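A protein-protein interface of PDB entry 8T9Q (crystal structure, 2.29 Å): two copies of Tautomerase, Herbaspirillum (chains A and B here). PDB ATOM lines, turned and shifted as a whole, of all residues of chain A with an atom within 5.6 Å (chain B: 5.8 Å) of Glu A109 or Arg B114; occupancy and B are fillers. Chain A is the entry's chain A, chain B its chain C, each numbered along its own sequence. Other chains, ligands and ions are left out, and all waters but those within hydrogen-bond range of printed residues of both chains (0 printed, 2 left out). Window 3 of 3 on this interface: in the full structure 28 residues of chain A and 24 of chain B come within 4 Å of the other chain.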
ATOM      1  N   GLY A  70     -21.942 -16.400  16.656  1.00  0.00           N
ATOM      2  CA  GLY A  70     -22.180 -16.901  15.297  1.00  0.00           C
ATOM      3  C   GLY A  70     -22.857 -15.827  14.514  1.00  0.00           C
ATOM      4  O   GLY A  70     -23.936 -15.462  14.931  1.00  0.00           O
ATOM      5  N   PRO A  72     -24.422 -15.431  10.987  1.00  0.00           N
ATOM      6  CA  PRO A  72     -24.858 -15.803   9.650  1.00  0.00           C
ATOM      7  C   PRO A  72     -25.767 -14.787   8.967  1.00  0.00           C
ATOM      8  O   PRO A  72     -26.313 -13.869   9.596  1.00  0.00           O
ATOM      9  CB  PRO A  72     -25.650 -17.074   9.980  1.00  0.00           C
ATOM     10  CG  PRO A  72     -26.410 -16.677  11.229  1.00  0.00           C
ATOM     11  CD  PRO A  72     -25.451 -15.771  11.987  1.00  0.00           C
ATOM     12  N   PRO A  73     -25.933 -14.937   7.635  1.00  0.00           N
ATOM     13  CA  PRO A  73     -26.994 -14.250   6.906  1.00  0.00           C
ATOM     14  C   PRO A  73     -28.346 -14.790   7.395  1.00  0.00           C
ATOM     15  O   PRO A  73     -28.410 -15.925   7.824  1.00  0.00           O
ATOM     16  CB  PRO A  73     -26.710 -14.540   5.420  1.00  0.00           C
ATOM     17  CG  PRO A  73     -25.311 -15.127   5.400  1.00  0.00           C
ATOM     18  CD  PRO A  73     -25.093 -15.761   6.757  1.00  0.00           C
ATOM     19  N   SER A  74     -29.388 -13.958   7.313  1.00  0.00           N
ATOM     20  CA  SER A  74     -30.722 -14.158   7.939  1.00  0.00           C
ATOM     21  C   SER A  74     -31.667 -14.873   6.971  1.00  0.00           C
ATOM     22  O   SER A  74     -32.368 -14.197   6.201  1.00  0.00           O
ATOM     23  CB  SER A  74     -31.314 -12.853   8.389  1.00  0.00           C
ATOM     24  OG  SER A  74     -32.681 -13.006   8.748  1.00  0.00           O
ATOM     25  N   LEU A  75     -31.703 -16.193   7.061  1.00  0.00           N
ATOM     26  CA  LEU A  75     -32.758 -17.050   6.477  1.00  0.00           C
ATOM     27  C   LEU A  75     -33.125 -18.091   7.528  1.00  0.00           C
ATOM     28  O   LEU A  75     -34.254 -18.614   7.469  1.00  0.00           O
ATOM     29  CB  LEU A  75     -32.211 -17.689   5.199  1.00  0.00           C
ATOM     30  CG  LEU A  75     -30.736 -18.091   5.268  1.00  0.00           C
ATOM     31  CD1 LEU A  75     -30.574 -19.602   5.229  1.00  0.00           C
ATOM     32  CD2 LEU A  75     -29.941 -17.430   4.149  1.00  0.00           C
ATOM     33  N   SER A  76     -32.206 -18.346   8.467  1.00  0.00           N
ATOM     34  CA  SER A  76     -32.203 -19.538   9.340  1.00  0.00           C
ATOM     35  C   SER A  76     -33.489 -19.564  10.158  1.00  0.00           C
ATOM     36  O   SER A  76     -33.840 -18.531  10.779  1.00  0.00           O
ATOM     37  CB  SER A  76     -30.997 -19.594  10.230  1.00  0.00           C
ATOM     38  OG  SER A  76     -29.905 -20.168   9.534  1.00  0.00           O
ATOM     39  N   THR A  81     -31.446 -23.132  14.233  1.00  0.00           N
ATOM     40  CA  THR A  81     -30.737 -22.231  15.178  1.00  0.00           C
ATOM     41  C   THR A  81     -30.533 -22.985  16.485  1.00  0.00           C
ATOM     42  O   THR A  81     -29.397 -22.983  16.985  1.00  0.00           O
ATOM     43  CB  THR A  81     -31.514 -20.930  15.369  1.00  0.00           C
ATOM     44  OG1 THR A  81     -32.749 -21.307  15.971  1.00  0.00           O
ATOM     45  CG2 THR A  81     -31.734 -20.208  14.053  1.00  0.00           C
ATOM     46  N   PHE A  82     -31.583 -23.649  16.983  1.00  0.00           N
ATOM     47  CA  PHE A  82     -31.532 -24.456  18.233  1.00  0.00           C
ATOM     48  C   PHE A  82     -30.566 -25.616  18.025  1.00  0.00           C
ATOM     49  O   PHE A  82     -29.757 -25.904  18.932  1.00  0.00           O
ATOM     50  CB  PHE A  82     -32.920 -24.936  18.658  1.00  0.00           C
ATOM     51  CG  PHE A  82     -33.843 -23.798  18.993  1.00  0.00           C
ATOM     52  CD1 PHE A  82     -33.592 -22.965  20.082  1.00  0.00           C
ATOM     53  CD2 PHE A  82     -34.920 -23.507  18.170  1.00  0.00           C
ATOM     54  CE1 PHE A  82     -34.428 -21.890  20.356  1.00  0.00           C
ATOM     55  CE2 PHE A  82     -35.764 -22.442  18.460  1.00  0.00           C
ATOM     56  CZ  PHE A  82     -35.522 -21.640  19.556  1.00  0.00           C
ATOM     57  N   THR A 105     -23.800 -19.566  23.787  1.00  0.00           N
ATOM     58  CA  THR A 105     -23.716 -19.330  22.335  1.00  0.00           C
ATOM     59  C   THR A 105     -24.638 -18.172  21.997  1.00  0.00           C
ATOM     60  O   THR A 105     -25.683 -18.083  22.610  1.00  0.00           O
ATOM     61  CB  THR A 105     -24.048 -20.589  21.540  1.00  0.00           C
ATOM     62  OG1 THR A 105     -22.946 -21.466  21.778  1.00  0.00           O
ATOM     63  CG2 THR A 105     -24.243 -20.303  20.065  1.00  0.00           C
ATOM     64  N   VAL A 106     -24.207 -17.331  21.063  1.00  0.00           N
ATOM     65  CA  VAL A 106     -24.889 -16.083  20.653  1.00  0.00           C
ATOM     66  C   VAL A 106     -25.085 -16.186  19.140  1.00  0.00           C
ATOM     67  O   VAL A 106     -24.102 -16.463  18.391  1.00  0.00           O
ATOM     68  CB  VAL A 106     -24.059 -14.861  21.088  1.00  0.00           C
ATOM     69  CG1 VAL A 106     -24.486 -13.585  20.384  1.00  0.00           C
ATOM     70  CG2 VAL A 106     -24.095 -14.678  22.596  1.00  0.00           C
ATOM     71  N   GLY A 107     -26.326 -16.015  18.705  1.00  0.00           N
ATOM     72  CA  GLY A 107     -26.683 -16.027  17.282  1.00  0.00           C
ATOM     73  C   GLY A 107     -26.977 -14.626  16.845  1.00  0.00           C
ATOM     74  O   GLY A 107     -27.930 -14.050  17.377  1.00  0.00           O
ATOM     75  N   ILE A 108     -26.215 -14.120  15.885  1.00  0.00           N
ATOM     76  CA  ILE A 108     -26.400 -12.742  15.356  1.00  0.00           C
ATOM     77  C   ILE A 108     -26.887 -12.842  13.911  1.00  0.00           C
ATOM     78  O   ILE A 108     -26.073 -13.191  13.051  1.00  0.00           O
ATOM     79  CB  ILE A 108     -25.094 -11.920  15.456  1.00  0.00           C
ATOM     80  CG1 ILE A 108     -24.337 -12.190  16.768  1.00  0.00           C
ATOM     81  CG2 ILE A 108     -25.415 -10.448  15.271  1.00  0.00           C
ATOM     82  CD1 ILE A 108     -22.923 -11.647  16.802  1.00  0.00           C
ATOM     83  N   GLU A 109     -28.126 -12.425  13.650  1.00  0.00           N
ATOM     84  CA  GLU A 109     -28.672 -12.342  12.275  1.00  0.00           C
ATOM     85  C   GLU A 109     -28.200 -11.032  11.610  1.00  0.00           C
ATOM     86  O   GLU A 109     -28.304  -9.923  12.176  1.00  0.00           O
ATOM     87  CB  GLU A 109     -30.186 -12.574  12.300  1.00  0.00           C
ATOM     88  CG  GLU A 109     -30.565 -14.054  12.202  1.00  0.00           C
ATOM     89  CD  GLU A 109     -31.958 -14.357  11.663  1.00  0.00           C
ATOM     90  OE1 GLU A 109     -32.073 -15.209  10.734  1.00  0.00           O
ATOM     91  OE2 GLU A 109     -32.934 -13.747  12.161  1.00  0.00           O
ATOM     92  N   ARG A 110     -27.667 -11.155  10.411  1.00  0.00           N
ATOM     93  CA  ARG A 110     -27.214 -10.007   9.586  1.00  0.00           C
ATOM     94  C   ARG A 110     -27.686 -10.256   8.155  1.00  0.00           C
ATOM     95  O   ARG A 110     -27.146 -11.182   7.582  1.00  0.00           O
ATOM     96  CB  ARG A 110     -25.684  -9.952   9.648  1.00  0.00           C
ATOM     97  CG  ARG A 110     -25.122  -9.488  10.987  1.00  0.00           C
ATOM     98  CD  ARG A 110     -23.969 -10.330  11.498  1.00  0.00           C
ATOM     99  NE  ARG A 110     -23.576  -9.853  12.823  1.00  0.00           N
ATOM    100  CZ  ARG A 110     -22.342  -9.850  13.332  1.00  0.00           C
ATOM    101  NH1 ARG A 110     -21.310 -10.305  12.638  1.00  0.00           N
ATOM    102  NH2 ARG A 110     -22.135  -9.367  14.545  1.00  0.00           N
ATOM    103  N   ALA A 111     -28.601  -9.483   7.557  1.00  0.00           N
ATOM    104  CA  ALA A 111     -28.862  -9.679   6.107  1.00  0.00           C
ATOM    105  C   ALA A 111     -29.450  -8.461   5.398  1.00  0.00           C
ATOM    106  O   ALA A 111     -30.671  -8.429   5.194  1.00  0.00           O
ATOM    107  CB  ALA A 111     -29.759 -10.875   5.905  1.00  0.00           C
ATOM    108  N   ARG B 110     -30.101  -9.891  21.653  1.00  0.00           N
ATOM    109  CA  ARG B 110     -30.155 -11.217  21.000  1.00  0.00           C
ATOM    110  C   ARG B 110     -31.497 -11.868  21.392  1.00  0.00           C
ATOM    111  O   ARG B 110     -31.803 -11.906  22.619  1.00  0.00           O
ATOM    112  CB  ARG B 110     -28.930 -12.022  21.455  1.00  0.00           C
ATOM    113  CG  ARG B 110     -27.645 -11.786  20.665  1.00  0.00           C
ATOM    114  CD  ARG B 110     -27.043 -10.405  20.795  1.00  0.00           C
ATOM    115  NE  ARG B 110     -25.599 -10.459  20.991  1.00  0.00           N
ATOM    116  CZ  ARG B 110     -24.678 -10.189  20.064  1.00  0.00           C
ATOM    117  NH1 ARG B 110     -23.391 -10.280  20.365  1.00  0.00           N
ATOM    118  NH2 ARG B 110     -25.034  -9.840  18.838  1.00  0.00           N
ATOM    119  N   ALA B 111     -32.299 -12.348  20.428  1.00  0.00           N
ATOM    120  CA  ALA B 111     -33.632 -12.951  20.702  1.00  0.00           C
ATOM    121  C   ALA B 111     -33.435 -14.246  21.491  1.00  0.00           C
ATOM    122  O   ALA B 111     -32.387 -14.894  21.292  1.00  0.00           O
ATOM    123  CB  ALA B 111     -34.398 -13.189  19.424  1.00  0.00           C
ATOM    124  N   GLU B 112     -34.375 -14.570  22.389  1.00  0.00           N
ATOM    125  CA  GLU B 112     -34.453 -15.855  23.148  1.00  0.00           C
ATOM    126  C   GLU B 112     -34.257 -17.073  22.226  1.00  0.00           C
ATOM    127  O   GLU B 112     -33.618 -18.049  22.667  1.00  0.00           O
ATOM    128  CB  GLU B 112     -35.796 -15.938  23.869  1.00  0.00           C
ATOM    129  CG  GLU B 112     -36.953 -15.384  23.054  1.00  0.00           C
ATOM    130  CD  GLU B 112     -38.327 -15.844  23.485  1.00  0.00           C
ATOM    131  OE1 GLU B 112     -38.411 -16.474  24.562  1.00  0.00           O
ATOM    132  OE2 GLU B 112     -39.315 -15.568  22.743  1.00  0.00           O
ATOM    133  N   VAL B 113     -34.773 -17.030  20.993  1.00  0.00           N
ATOM    134  CA  VAL B 113     -34.527 -18.096  19.973  1.00  0.00           C
ATOM    135  C   VAL B 113     -33.047 -18.120  19.548  1.00  0.00           C
ATOM    136  O   VAL B 113     -32.655 -19.096  18.863  1.00  0.00           O
ATOM    137  CB  VAL B 113     -35.452 -17.958  18.746  1.00  0.00           C
ATOM    138  CG1 VAL B 113     -36.919 -18.035  19.129  1.00  0.00           C
ATOM    139  CG2 VAL B 113     -35.182 -16.707  17.936  1.00  0.00           C
ATOM    140  N   ARG B 114     -32.240 -17.114  19.912  1.00  0.00           N
ATOM    141  CA  ARG B 114     -30.860 -16.985  19.365  1.00  0.00           C
ATOM    142  C   ARG B 114     -29.809 -17.040  20.471  1.00  0.00           C
ATOM    143  O   ARG B 114     -28.617 -17.133  20.130  1.00  0.00           O
ATOM    144  CB  ARG B 114     -30.765 -15.720  18.510  1.00  0.00           C
ATOM    145  CG  ARG B 114     -31.760 -15.726  17.360  1.00  0.00           C
ATOM    146  CD  ARG B 114     -31.499 -14.662  16.330  1.00  0.00           C
ATOM    147  NE  ARG B 114     -32.738 -14.088  15.829  1.00  0.00           N
ATOM    148  CZ  ARG B 114     -33.504 -14.604  14.864  1.00  0.00           C
ATOM    149  NH1 ARG B 114     -34.612 -13.969  14.522  1.00  0.00           N
ATOM    150  NH2 ARG B 114     -33.180 -15.738  14.251  1.00  0.00           N
ATOM    151  N   VAL B 115     -30.215 -17.024  21.741  1.00  0.00           N
ATOM    152  CA  VAL B 115     -29.259 -17.093  22.880  1.00  0.00           C
ATOM    153  C   VAL B 115     -29.263 -18.525  23.409  1.00  0.00           C
ATOM    154  O   VAL B 115     -30.334 -18.993  23.806  1.00  0.00           O
ATOM    155  CB  VAL B 115     -29.561 -16.048  23.979  1.00  0.00           C
ATOM    156  CG1 VAL B 115     -31.003 -16.065  24.472  1.00  0.00           C
ATOM    157  CG2 VAL B 115     -28.602 -16.171  25.161  1.00  0.00           C
ATOM    158  N   ILE B 116     -28.108 -19.195  23.417  1.00  0.00           N
ATOM    159  CA  ILE B 116     -28.012 -20.562  24.002  1.00  0.00           C
ATOM    160  C   ILE B 116     -27.156 -20.514  25.281  1.00  0.00           C
ATOM    161  O   ILE B 116     -25.937 -20.255  25.195  1.00  0.00           O
ATOM    162  CB  ILE B 116     -27.563 -21.564  22.914  1.00  0.00           C
ATOM    163  CG1 ILE B 116     -28.773 -22.225  22.241  1.00  0.00           C
ATOM    164  CG2 ILE B 116     -26.596 -22.611  23.453  1.00  0.00           C
ATOM    165  CD1 ILE B 116     -29.315 -21.488  21.025  1.00  0.00           C
ATOM    166  N   PRO B 121     -31.885 -23.010  24.680  1.00  0.00           N
ATOM    167  CA  PRO B 121     -32.093 -21.579  24.472  1.00  0.00           C
ATOM    168  C   PRO B 121     -32.854 -21.030  25.678  1.00  0.00           C
ATOM    169  O   PRO B 121     -33.315 -21.842  26.461  1.00  0.00           O
ATOM    170  CB  PRO B 121     -33.004 -21.542  23.252  1.00  0.00           C
ATOM    171  CG  PRO B 121     -33.867 -22.750  23.495  1.00  0.00           C
ATOM    172  CD  PRO B 121     -32.877 -23.809  23.945  1.00  0.00           C
ATOM    173  N   THR B 123     -35.706 -19.596  25.190  1.00  0.00           N
ATOM    174  CA  THR B 123     -37.117 -19.774  24.744  1.00  0.00           C
ATOM    175  C   THR B 123     -37.661 -21.057  25.379  1.00  0.00           C
ATOM    176  O   THR B 123     -38.648 -20.958  26.128  1.00  0.00           O
ATOM    177  CB  THR B 123     -37.260 -19.795  23.216  1.00  0.00           C
ATOM    178  OG1 THR B 123     -36.522 -18.708  22.656  1.00  0.00           O
ATOM    179  CG2 THR B 123     -38.702 -19.704  22.762  1.00  0.00           C
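The backbone carbonyl oxygen of Ile B116 sits at hydrogen-bond distance from the backbone NH of Thr A105, 2.7 Å away.
The backbone NH (N) of Gly A107 lies within hydrogen-bond range of the backbone carbonyl oxygen (O) of Arg B114, 2.9 Å away.
The guanidinium group of Arg B114 is in salt-bridge range of the side-chain carboxylate of Glu A109, at 2.9 Å.
Of the 9 printed residues of chain B, 6 touch a printed residue of chain A.
Hydrophobic or aromatic side chains of chain B that line the printed part of chain A: Val B113, Ile B116 and Pro B121.
Of the 15 printed residues of chain A, 7 touch a printed residue of chain B.
Hydrophobic or aromatic side chains of chain A within 4 Å of the printed part of chain B: Phe A82, Val A106 and Ile A108.
Among the printed residues, Asp or Glu carboxylates within 4 Å of a Lys or Arg side-chain nitrogen of the other chain: Glu A109 with Arg B114 (2.9 Å).
The backbone carbonyl oxygen of Val A106 sits at hydrogen-bond distance from the backbone NH of Gly A70 (2.8 Å).
The backbone carbonyl oxygen (O) of Gly A70 is in hydrogen-bond range of the backbone NH (N) of Ile A108.
OE1 of Glu A109 sits at hydrogen-bond distance from OG of Ser A74, 3.0 Å away.
N of Val B113 is in hydrogen-bond range of OG1 of Thr B123, at 2.9 Å.
2 positions are printed for both chains.
Of the 11 pairs that touch across the chains among the printed residues, none has its exchanged pair printed and touching as well.
Gly A70 touches none of the printed residues of chain B.
Printed residues of chain B within 4 Å of Phe A82: Val B113 and Pro B121.
Printed residues of chain B within 4 Å of Thr A105: Arg B114, Val B115 and Ile B116.
Of the printed residues of chain B, Val A106 touches Arg B110 (3.4 Å) and Arg B114 (3.8 Å).
Printed residues of chain B within 4 Å of Gly A107: Arg B114.
Of chain B, only Arg B114 (2.9 Å) comes within 4 Å of Glu A109.
Printed residues of chain A within 4 Å of Ile B116: Thr A105.
The nearest residue of chain A that does not touch Arg B114 is Ser A76 (4.5 Å).
O of Val B113 touches OG1 of Thr A81, at 3.6 Å.
CE1 of Phe A82 touches O of Val B113 (3.6 Å).
CE1 of Phe A82 touches CB of Pro B121, 3.2 Å away.
Arg B114 touches Thr A105 (O to O, 3.96 Å).
Val B115 touches Thr A105.
CG1 of Val A106 touches NE of Arg B110, at 3.4 Å.
Arg B114 touches Val A106 (O to C, 3.8 Å).
Arg B110 touches Ile A108 (NH2 to CG1, 3.2 Å).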
